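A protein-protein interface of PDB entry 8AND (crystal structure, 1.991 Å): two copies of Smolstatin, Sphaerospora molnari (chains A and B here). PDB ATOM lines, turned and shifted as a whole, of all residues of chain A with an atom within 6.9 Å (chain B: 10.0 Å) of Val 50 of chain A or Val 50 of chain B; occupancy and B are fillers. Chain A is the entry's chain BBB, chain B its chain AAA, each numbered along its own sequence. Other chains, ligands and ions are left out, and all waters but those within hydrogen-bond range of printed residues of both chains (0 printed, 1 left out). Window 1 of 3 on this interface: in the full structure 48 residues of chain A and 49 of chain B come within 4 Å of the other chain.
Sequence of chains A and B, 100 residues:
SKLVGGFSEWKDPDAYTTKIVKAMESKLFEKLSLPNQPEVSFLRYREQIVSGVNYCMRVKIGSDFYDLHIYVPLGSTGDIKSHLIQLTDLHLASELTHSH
Of the 10 printed residues of chain A, 7 touch a printed residue of chain B.
Of the 19 printed residues of chain B, 9 touch a printed residue of chain A.
Among the printed residues, no Asp or Glu carboxylate lies within 4 Å of a Lys or Arg side-chain nitrogen of the other chain.
O of Gly 52 of chain B sits at hydrogen-bond distance from N of Val 50 of chain A.
The backbone carbonyl oxygen (O) of Asn 54 of chain A lies within hydrogen-bond range of the backbone NH (N) of Gln 48 of chain B, at 2.8 Å.
The backbone carbonyl oxygen (O) of Gly 52 of chain A sits at hydrogen-bond distance from the backbone NH (N) of Val 50 of chain B (2.9 Å).
O of Asn 54 of chain B sits at hydrogen-bond distance from N of Gln 48 of chain A, at 2.8 Å.
Gln 48 of chain A touches Asn 54 of chain B, and with the chains exchanged Asn 54 of chain A touches Gln 48 of chain B.
Ile 49 of chain A touches Gly 52 of chain B, and with the chains exchanged Gly 52 of chain A touches Ile 49 of chain B.
Val 50 of chain A touches Asn 54 of chain B, and with the chains exchanged Asn 54 of chain A touches Val 50 of chain B.
Ser 51 of chain A touches its own counterpart, Ser 51 of chain B.
Among the printed residues, merely in contact across the chains: Gln 48 of chain A with Val 53 of chain B (3.5 Å), Ile 49 of chain A with Gly 52 of chain B (3.8 Å), Val 50 of chain A with Val 50 of chain B (3.95 Å), Val 50 of chain A with Ser 51 of chain B (3.4 Å), Val 50 of chain A with Asn 54 of chain B (3.4 Å), Ser 51 of chain A with Val 50 of chain B (3.4 Å), Ser 51 of chain A with Ser 51 of chain B (3.5 Å), Gly 52 of chain A with Ile 49 of chain B (3.8 Å), Val 53 of chain A with Glu 47 of chain B (3.8 Å), Val 53 of chain A with Gln 48 of chain B (3.5 Å), Asn 54 of chain A with Phe 7 of chain B (3.8 Å), Asn 54 of chain A with Glu 47 of chain B (3.3 Å) and Asn 54 of chain A with Val 50 of chain B (3.6 Å).
Printed residues of chain B within 4 Å of Val 50 of chain A: Val 50, Ser 51, Gly 52 and Asn 54.
Of the printed residues of chain A, Val 50 of chain B touches Val 50, Ser 51, Gly 52 and Asn 54.
Of the printed residues of chain A, Ser 51 of chain B touches Val 50 (3.4 Å) and Ser 51 (3.5 Å).
Of the printed residues of chain B, Ser 51 of chain A touches Val 50 (3.4 Å) and Ser 51 (3.5 Å).
Of the printed residues of chain B, Gln 48 of chain A touches Val 53 (3.5 Å) and Asn 54 (2.8 Å).
Of the printed residues of chain A, Phe 7 of chain B touches Asn 54.
Printed residues of chain B within 4 Å of Val 53 of chain A: Glu 47 and Gln 48.
Gly 5 of chain B touches none of the printed residues of chain A.
The nearest printed residue of chain A that does not touch Val 50 of chain B is Val 53 of chain A (4.7 Å).
The nearest printed residue of chain A that does not touch Glu 47 of chain B is Gly 52 of chain A (8.0 Å).
The backbone NH of Gly 52 of chain A lies close to the side-chain hydroxyl of Tyr 71 of chain A.
The backbone carbonyl oxygen (O) of Ser 51 of chain A is in hydrogen-bond range of the backbone NH (N) of Leu 74 of chain A, 2.9 Å away.
The side-chain hydroxyl (OH) of Tyr 71 of chain B lies within hydrogen-bond range of the backbone carbonyl oxygen (O) of Ser 51 of chain B (3.1 Å).
O of Ser 51 of chain A lies within hydrogen-bond range of OH of Tyr 71 of chain A (3.2 Å).
The side-chain amide nitrogen (NE2) of Gln 48 of chain A lies close to the backbone NH (N) of Gly 5 of chain A (3.3 Å).
The backbone NH of Leu 74 of chain B lies within hydrogen-bond range of the backbone carbonyl oxygen of Ser 51 of chain B (2.9 Å).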
ATOM      1  N   GLY A   5      15.182 -30.527   3.265  1.00  0.00           N
ATOM      2  CA  GLY A   5      14.589 -31.901   3.360  1.00  0.00           C
ATOM      3  C   GLY A   5      14.066 -32.242   4.747  1.00  0.00           C
ATOM      4  O   GLY A   5      13.759 -33.438   4.972  1.00  0.00           O
ATOM      5  N   GLN A  48       7.974 -27.088   5.490  1.00  0.00           N
ATOM      6  CA  GLN A  48       9.387 -27.147   5.055  1.00  0.00           C
ATOM      7  C   GLN A  48       9.561 -26.083   3.980  1.00  0.00           C
ATOM      8  O   GLN A  48       8.926 -26.215   2.918  1.00  0.00           O
ATOM      9  CB  GLN A  48       9.714 -28.537   4.528  1.00  0.00           C
ATOM     10  CG  GLN A  48      10.944 -28.619   3.638  1.00  0.00           C
ATOM     11  CD  GLN A  48      10.935 -29.852   2.768  1.00  0.00           C
ATOM     12  OE1 GLN A  48      10.116 -30.004   1.869  1.00  0.00           O
ATOM     13  NE2 GLN A  48      11.867 -30.754   3.022  1.00  0.00           N
ATOM     14  N   ILE A  49      10.338 -25.053   4.274  1.00  0.00           N
ATOM     15  CA  ILE A  49      10.723 -24.052   3.249  1.00  0.00           C
ATOM     16  C   ILE A  49      11.579 -24.770   2.206  1.00  0.00           C
ATOM     17  O   ILE A  49      12.462 -25.566   2.575  1.00  0.00           O
ATOM     18  CB  ILE A  49      11.481 -22.865   3.849  1.00  0.00           C
ATOM     19  CG1 ILE A  49      10.586 -21.941   4.675  1.00  0.00           C
ATOM     20  CG2 ILE A  49      12.147 -22.090   2.728  1.00  0.00           C
ATOM     21  CD1 ILE A  49       9.664 -22.636   5.658  1.00  0.00           C
ATOM     22  N   VAL A  50      11.327 -24.494   0.935  1.00  0.00           N
ATOM     23  CA  VAL A  50      12.169 -25.011  -0.179  1.00  0.00           C
ATOM     24  C   VAL A  50      12.468 -23.842  -1.115  1.00  0.00           C
ATOM     25  O   VAL A  50      11.511 -23.278  -1.707  1.00  0.00           O
ATOM     26  CB  VAL A  50      11.501 -26.173  -0.924  1.00  0.00           C
ATOM     27  CG1 VAL A  50      12.319 -26.585  -2.129  1.00  0.00           C
ATOM     28  CG2 VAL A  50      11.272 -27.366  -0.008  1.00  0.00           C
ATOM     29  N   SER A  51      13.741 -23.480  -1.206  1.00  0.00           N
ATOM     30  CA  SER A  51      14.178 -22.328  -2.014  1.00  0.00           C
ATOM     31  C   SER A  51      15.473 -22.683  -2.728  1.00  0.00           C
ATOM     32  O   SER A  51      16.352 -23.300  -2.096  1.00  0.00           O
ATOM     33  CB  SER A  51      14.351 -21.148  -1.155  1.00  0.00           C
ATOM     34  OG  SER A  51      14.535 -20.000  -1.955  1.00  0.00           O
ATOM     35  N   GLY A  52      15.597 -22.269  -3.984  1.00  0.00           N
ATOM     36  CA  GLY A  52      16.848 -22.477  -4.731  1.00  0.00           C
ATOM     37  C   GLY A  52      16.707 -22.011  -6.159  1.00  0.00           C
ATOM     38  O   GLY A  52      15.635 -21.399  -6.531  1.00  0.00           O
ATOM     39  N   VAL A  53      17.727 -22.270  -6.965  1.00  0.00           N
ATOM     40  CA  VAL A  53      17.695 -21.881  -8.400  1.00  0.00           C
ATOM     41  C   VAL A  53      18.036 -23.124  -9.191  1.00  0.00           C
ATOM     42  O   VAL A  53      19.058 -23.802  -8.871  1.00  0.00           O
ATOM     43  CB  VAL A  53      18.648 -20.719  -8.712  1.00  0.00           C
ATOM     44  CG1 VAL A  53      18.626 -20.374 -10.190  1.00  0.00           C
ATOM     45  CG2 VAL A  53      18.375 -19.494  -7.847  1.00  0.00           C
ATOM     46  N   ASN A  54      17.221 -23.428 -10.197  1.00  0.00           N
ATOM     47  CA  ASN A  54      17.611 -24.445 -11.194  1.00  0.00           C
ATOM     48  C   ASN A  54      18.364 -23.743 -12.309  1.00  0.00           C
ATOM     49  O   ASN A  54      17.889 -22.696 -12.799  1.00  0.00           O
ATOM     50  CB  ASN A  54      16.431 -25.208 -11.787  1.00  0.00           C
ATOM     51  CG  ASN A  54      15.795 -26.133 -10.779  1.00  0.00           C
ATOM     52  OD1 ASN A  54      16.428 -27.094 -10.328  1.00  0.00           O
ATOM     53  ND2 ASN A  54      14.555 -25.831 -10.439  1.00  0.00           N
ATOM     54  N   TYR A  71      20.940 -27.886  -9.605  1.00  0.00           N
ATOM     55  CA  TYR A  71      20.099 -27.220  -8.582  1.00  0.00           C
ATOM     56  C   TYR A  71      20.968 -26.673  -7.460  1.00  0.00           C
ATOM     57  O   TYR A  71      21.680 -27.447  -6.817  1.00  0.00           O
ATOM     58  CB  TYR A  71      19.070 -28.188  -8.003  1.00  0.00           C
ATOM     59  CG  TYR A  71      18.222 -27.533  -6.958  1.00  0.00           C
ATOM     60  CD1 TYR A  71      17.292 -26.558  -7.297  1.00  0.00           C
ATOM     61  CD2 TYR A  71      18.357 -27.875  -5.616  1.00  0.00           C
ATOM     62  CE1 TYR A  71      16.478 -25.981  -6.332  1.00  0.00           C
ATOM     63  CE2 TYR A  71      17.559 -27.290  -4.652  1.00  0.00           C
ATOM     64  CZ  TYR A  71      16.619 -26.338  -5.003  1.00  0.00           C
ATOM     65  OH  TYR A  71      15.870 -25.745  -4.028  1.00  0.00           O
ATOM     66  N   LEU A  74      19.090 -22.433  -1.828  1.00  0.00           N
ATOM     67  CA  LEU A  74      19.316 -21.198  -1.056  1.00  0.00           C
ATOM     68  C   LEU A  74      20.393 -21.445   0.019  1.00  0.00           C
ATOM     69  O   LEU A  74      20.348 -22.467   0.713  1.00  0.00           O
ATOM     70  CB  LEU A  74      18.003 -20.774  -0.393  1.00  0.00           C
ATOM     71  CG  LEU A  74      18.108 -19.490   0.435  1.00  0.00           C
ATOM     72  CD1 LEU A  74      18.305 -18.287  -0.478  1.00  0.00           C
ATOM     73  CD2 LEU A  74      16.861 -19.311   1.306  1.00  0.00           C
ATOM     74  N   GLY B   5      10.400 -22.682 -20.094  1.00  0.00           N
ATOM     75  CA  GLY B   5       9.205 -23.039 -19.272  1.00  0.00           C
ATOM     76  C   GLY B   5       9.398 -22.696 -17.804  1.00  0.00           C
ATOM     77  O   GLY B   5       9.462 -23.625 -16.982  1.00  0.00           O
ATOM     78  N   GLY B   6       9.444 -21.401 -17.491  1.00  0.00           N
ATOM     79  CA  GLY B   6       9.841 -20.872 -16.171  1.00  0.00           C
ATOM     80  C   GLY B   6      11.290 -20.412 -16.176  1.00  0.00           C
ATOM     81  O   GLY B   6      11.676 -19.642 -15.282  1.00  0.00           O
ATOM     82  N   PHE B   7      12.070 -20.842 -17.169  1.00  0.00           N
ATOM     83  CA  PHE B   7      13.503 -20.485 -17.289  1.00  0.00           C
ATOM     84  C   PHE B   7      13.641 -19.136 -17.984  1.00  0.00           C
ATOM     85  O   PHE B   7      12.871 -18.826 -18.904  1.00  0.00           O
ATOM     86  CB  PHE B   7      14.280 -21.562 -18.040  1.00  0.00           C
ATOM     87  CG  PHE B   7      14.606 -22.777 -17.214  1.00  0.00           C
ATOM     88  CD1 PHE B   7      13.666 -23.772 -17.017  1.00  0.00           C
ATOM     89  CD2 PHE B   7      15.837 -22.899 -16.604  1.00  0.00           C
ATOM     90  CE1 PHE B   7      13.966 -24.884 -16.250  1.00  0.00           C
ATOM     91  CE2 PHE B   7      16.145 -24.015 -15.846  1.00  0.00           C
ATOM     92  CZ  PHE B   7      15.212 -25.009 -15.669  1.00  0.00           C
ATOM     93  N   GLU B  47      18.314 -19.771 -16.053  1.00  0.00           N
ATOM     94  CA  GLU B  47      18.022 -20.013 -14.629  1.00  0.00           C
ATOM     95  C   GLU B  47      16.526 -19.924 -14.391  1.00  0.00           C
ATOM     96  O   GLU B  47      15.794 -19.271 -15.180  1.00  0.00           O
ATOM     97  CB  GLU B  47      18.764 -19.015 -13.764  1.00  0.00           C
ATOM     98  CG  GLU B  47      18.386 -17.587 -14.030  1.00  0.00           C
ATOM     99  CD  GLU B  47      19.084 -16.627 -13.096  1.00  0.00           C
ATOM    100  OE1 GLU B  47      20.133 -16.989 -12.571  1.00  0.00           O
ATOM    101  OE2 GLU B  47      18.584 -15.535 -12.893  1.00  0.00           O
ATOM    102  N   GLN B  48      16.105 -20.589 -13.335  1.00  0.00           N
ATOM    103  CA  GLN B  48      14.686 -20.643 -12.912  1.00  0.00           C
ATOM    104  C   GLN B  48      14.658 -20.639 -11.387  1.00  0.00           C
ATOM    105  O   GLN B  48      15.077 -21.628 -10.773  1.00  0.00           O
ATOM    106  CB  GLN B  48      14.036 -21.902 -13.478  1.00  0.00           C
ATOM    107  CG  GLN B  48      12.674 -22.203 -12.870  1.00  0.00           C
ATOM    108  CD  GLN B  48      12.260 -23.630 -13.117  1.00  0.00           C
ATOM    109  OE1 GLN B  48      12.868 -24.562 -12.606  1.00  0.00           O
ATOM    110  NE2 GLN B  48      11.227 -23.810 -13.925  1.00  0.00           N
ATOM    111  N   ILE B  49      14.272 -19.520 -10.806  1.00  0.00           N
ATOM    112  CA  ILE B  49      14.125 -19.424  -9.340  1.00  0.00           C
ATOM    113  C   ILE B  49      12.932 -20.283  -8.942  1.00  0.00           C
ATOM    114  O   ILE B  49      11.874 -20.200  -9.606  1.00  0.00           O
ATOM    115  CB  ILE B  49      13.953 -17.986  -8.894  1.00  0.00           C
ATOM    116  CG1 ILE B  49      15.158 -17.141  -9.305  1.00  0.00           C
ATOM    117  CG2 ILE B  49      13.707 -17.950  -7.395  1.00  0.00           C
ATOM    118  CD1 ILE B  49      14.942 -15.667  -9.106  1.00  0.00           C
ATOM    119  N   VAL B  50      13.104 -21.120  -7.921  1.00  0.00           N
ATOM    120  CA  VAL B  50      11.989 -21.951  -7.395  1.00  0.00           C
ATOM    121  C   VAL B  50      11.956 -21.787  -5.883  1.00  0.00           C
ATOM    122  O   VAL B  50      12.952 -22.171  -5.215  1.00  0.00           O
ATOM    123  CB  VAL B  50      12.122 -23.415  -7.817  1.00  0.00           C
ATOM    124  CG1 VAL B  50      11.039 -24.266  -7.181  1.00  0.00           C
ATOM    125  CG2 VAL B  50      12.064 -23.543  -9.328  1.00  0.00           C
ATOM    126  N   SER B  51      10.881 -21.210  -5.378  1.00  0.00           N
ATOM    127  CA  SER B  51      10.761 -20.884  -3.946  1.00  0.00           C
ATOM    128  C   SER B  51       9.321 -21.129  -3.505  1.00  0.00           C
ATOM    129  O   SER B  51       8.411 -20.783  -4.249  1.00  0.00           O
ATOM    130  CB  SER B  51      11.183 -19.484  -3.700  1.00  0.00           C
ATOM    131  OG  SER B  51      11.101 -19.204  -2.330  1.00  0.00           O
ATOM    132  N   GLY B  52       9.153 -21.651  -2.295  1.00  0.00           N
ATOM    133  CA  GLY B  52       7.816 -21.890  -1.726  1.00  0.00           C
ATOM    134  C   GLY B  52       7.921 -22.714  -0.466  1.00  0.00           C
ATOM    135  O   GLY B  52       9.066 -22.884   0.091  1.00  0.00           O
ATOM    136  N   VAL B  53       6.792 -23.242  -0.019  1.00  0.00           N
ATOM    137  CA  VAL B  53       6.746 -23.992   1.264  1.00  0.00           C
ATOM    138  C   VAL B  53       5.975 -25.274   1.022  1.00  0.00           C
ATOM    139  O   VAL B  53       4.853 -25.229   0.432  1.00  0.00           O
ATOM    140  CB  VAL B  53       6.141 -23.165   2.403  1.00  0.00           C
ATOM    141  CG1 VAL B  53       5.986 -23.998   3.655  1.00  0.00           C
ATOM    142  CG2 VAL B  53       6.964 -21.938   2.713  1.00  0.00           C
ATOM    143  N   ASN B  54       6.531 -26.388   1.481  1.00  0.00           N
ATOM    144  CA  ASN B  54       5.799 -27.670   1.481  1.00  0.00           C
ATOM    145  C   ASN B  54       5.101 -27.797   2.837  1.00  0.00           C
ATOM    146  O   ASN B  54       5.748 -27.583   3.890  1.00  0.00           O
ATOM    147  CB  ASN B  54       6.703 -28.876   1.239  1.00  0.00           C
ATOM    148  CG  ASN B  54       7.147 -29.013  -0.203  1.00  0.00           C
ATOM    149  OD1 ASN B  54       8.347 -29.103  -0.469  1.00  0.00           O
ATOM    150  ND2 ASN B  54       6.198 -29.048  -1.129  1.00  0.00           N
ATOM    151  N   TYR B  55       3.825 -28.100   2.803  1.00  0.00           N
ATOM    152  CA  TYR B  55       3.022 -28.304   4.023  1.00  0.00           C
ATOM    153  C   TYR B  55       2.613 -29.763   4.083  1.00  0.00           C
ATOM    154  O   TYR B  55       2.189 -30.310   3.063  1.00  0.00           O
ATOM    155  CB  TYR B  55       1.803 -27.402   4.057  1.00  0.00           C
ATOM    156  CG  TYR B  55       2.141 -25.950   4.183  1.00  0.00           C
ATOM    157  CD1 TYR B  55       2.407 -25.396   5.418  1.00  0.00           C
ATOM    158  CD2 TYR B  55       2.244 -25.137   3.058  1.00  0.00           C
ATOM    159  CE1 TYR B  55       2.756 -24.054   5.546  1.00  0.00           C
ATOM    160  CE2 TYR B  55       2.637 -23.816   3.173  1.00  0.00           C
ATOM    161  CZ  TYR B  55       2.866 -23.263   4.420  1.00  0.00           C
ATOM    162  OH  TYR B  55       3.208 -21.948   4.506  1.00  0.00           O
ATOM    163  N   ILE B  70       0.828 -30.270   0.460  1.00  0.00           N
ATOM    164  CA  ILE B  70       0.412 -29.076  -0.321  1.00  0.00           C
ATOM    165  C   ILE B  70       1.647 -28.224  -0.522  1.00  0.00           C
ATOM    166  O   ILE B  70       2.362 -27.953   0.459  1.00  0.00           O
ATOM    167  CB  ILE B  70      -0.704 -28.295   0.384  1.00  0.00           C
ATOM    168  CG1 ILE B  70      -1.979 -29.120   0.497  1.00  0.00           C
ATOM    169  CG2 ILE B  70      -0.948 -26.962  -0.317  1.00  0.00           C
ATOM    170  CD1 ILE B  70      -2.973 -28.566   1.467  1.00  0.00           C
ATOM    171  N   TYR B  71       1.876 -27.802  -1.750  1.00  0.00           N
ATOM    172  CA  TYR B  71       2.981 -26.883  -2.057  1.00  0.00           C
ATOM    173  C   TYR B  71       2.398 -25.497  -2.362  1.00  0.00           C
ATOM    174  O   TYR B  71       1.518 -25.355  -3.244  1.00  0.00           O
ATOM    175  CB  TYR B  71       3.827 -27.410  -3.210  1.00  0.00           C
ATOM    176  CG  TYR B  71       4.906 -26.455  -3.640  1.00  0.00           C
ATOM    177  CD1 TYR B  71       4.806 -25.767  -4.841  1.00  0.00           C
ATOM    178  CD2 TYR B  71       6.010 -26.214  -2.837  1.00  0.00           C
ATOM    179  CE1 TYR B  71       5.784 -24.872  -5.235  1.00  0.00           C
ATOM    180  CE2 TYR B  71       7.002 -25.335  -3.230  1.00  0.00           C
ATOM    181  CZ  TYR B  71       6.888 -24.668  -4.437  1.00  0.00           C
ATOM    182  OH  TYR B  71       7.838 -23.772  -4.836  1.00  0.00           O
ATOM    183  N   VAL B  72       2.892 -24.502  -1.646  1.00  0.00           N
ATOM    184  CA  VAL B  72       2.461 -23.093  -1.816  1.00  0.00           C
ATOM    185  C   VAL B  72       3.648 -22.312  -2.355  1.00  0.00           C
ATOM    186  O   VAL B  72       4.612 -22.071  -1.613  1.00  0.00           O
ATOM    187  CB  VAL B  72       1.958 -22.493  -0.500  1.00  0.00           C
ATOM    188  CG1 VAL B  72       1.490 -21.058  -0.722  1.00  0.00           C
ATOM    189  CG2 VAL B  72       0.873 -23.384   0.110  1.00  0.00           C
ATOM    190  N   PRO B  73       3.613 -21.894  -3.638  1.00  0.00           N
ATOM    191  CA  PRO B  73       4.728 -21.153  -4.209  1.00  0.00           C
ATOM    192  C   PRO B  73       4.819 -19.782  -3.546  1.00  0.00           C
ATOM    193  O   PRO B  73       3.817 -19.221  -3.134  1.00  0.00           O
ATOM    194  CB  PRO B  73       4.390 -21.012  -5.700  1.00  0.00           C
ATOM    195  CG  PRO B  73       3.319 -22.036  -5.932  1.00  0.00           C
ATOM    196  CD  PRO B  73       2.551 -22.127  -4.628  1.00  0.00           C
ATOM    197  N   LEU B  74       6.043 -19.292  -3.430  1.00  0.00           N
ATOM    198  CA  LEU B  74       6.246 -17.902  -2.952  1.00  0.00           C
ATOM    199  C   LEU B  74       5.366 -16.952  -3.780  1.00  0.00           C
ATOM    200  O   LEU B  74       5.221 -17.141  -5.001  1.00  0.00           O
ATOM    201  CB  LEU B  74       7.730 -17.551  -3.091  1.00  0.00           C
ATOM    202  CG  LEU B  74       8.108 -16.080  -3.192  1.00  0.00           C
ATOM    203  CD1 LEU B  74       8.045 -15.441  -1.818  1.00  0.00           C
ATOM    204  CD2 LEU B  74       9.506 -15.935  -3.779  1.00  0.00           C
ATOM    205  N   GLY B  75       4.791 -15.962  -3.123  1.00  0.00           N
ATOM    206  CA  GLY B  75       3.837 -15.038  -3.756  1.00  0.00           C
ATOM    207  C   GLY B  75       2.400 -15.523  -3.664  1.00  0.00           C
ATOM    208  O   GLY B  75       1.497 -14.705  -3.877  1.00  0.00           O
ATOM    209  N   GLN B  86      -0.559 -26.222  -5.052  1.00  0.00           N
ATOM    210  CA  GLN B  86      -0.587 -27.600  -5.613  1.00  0.00           C
ATOM    211  C   GLN B  86      -0.890 -28.614  -4.504  1.00  0.00           C
ATOM    212  O   GLN B  86      -0.216 -28.567  -3.457  1.00  0.00           O
ATOM    213  CB  GLN B  86       0.749 -27.938  -6.262  1.00  0.00           C
ATOM    214  CG  GLN B  86       1.177 -26.994  -7.382  1.00  0.00           C
ATOM    215  CD  GLN B  86       2.630 -27.169  -7.770  1.00  0.00           C
ATOM    216  OE1 GLN B  86       3.310 -28.115  -7.331  1.00  0.00           O
ATOM    217  NE2 GLN B  86       3.143 -26.240  -8.579  1.00  0.00           N
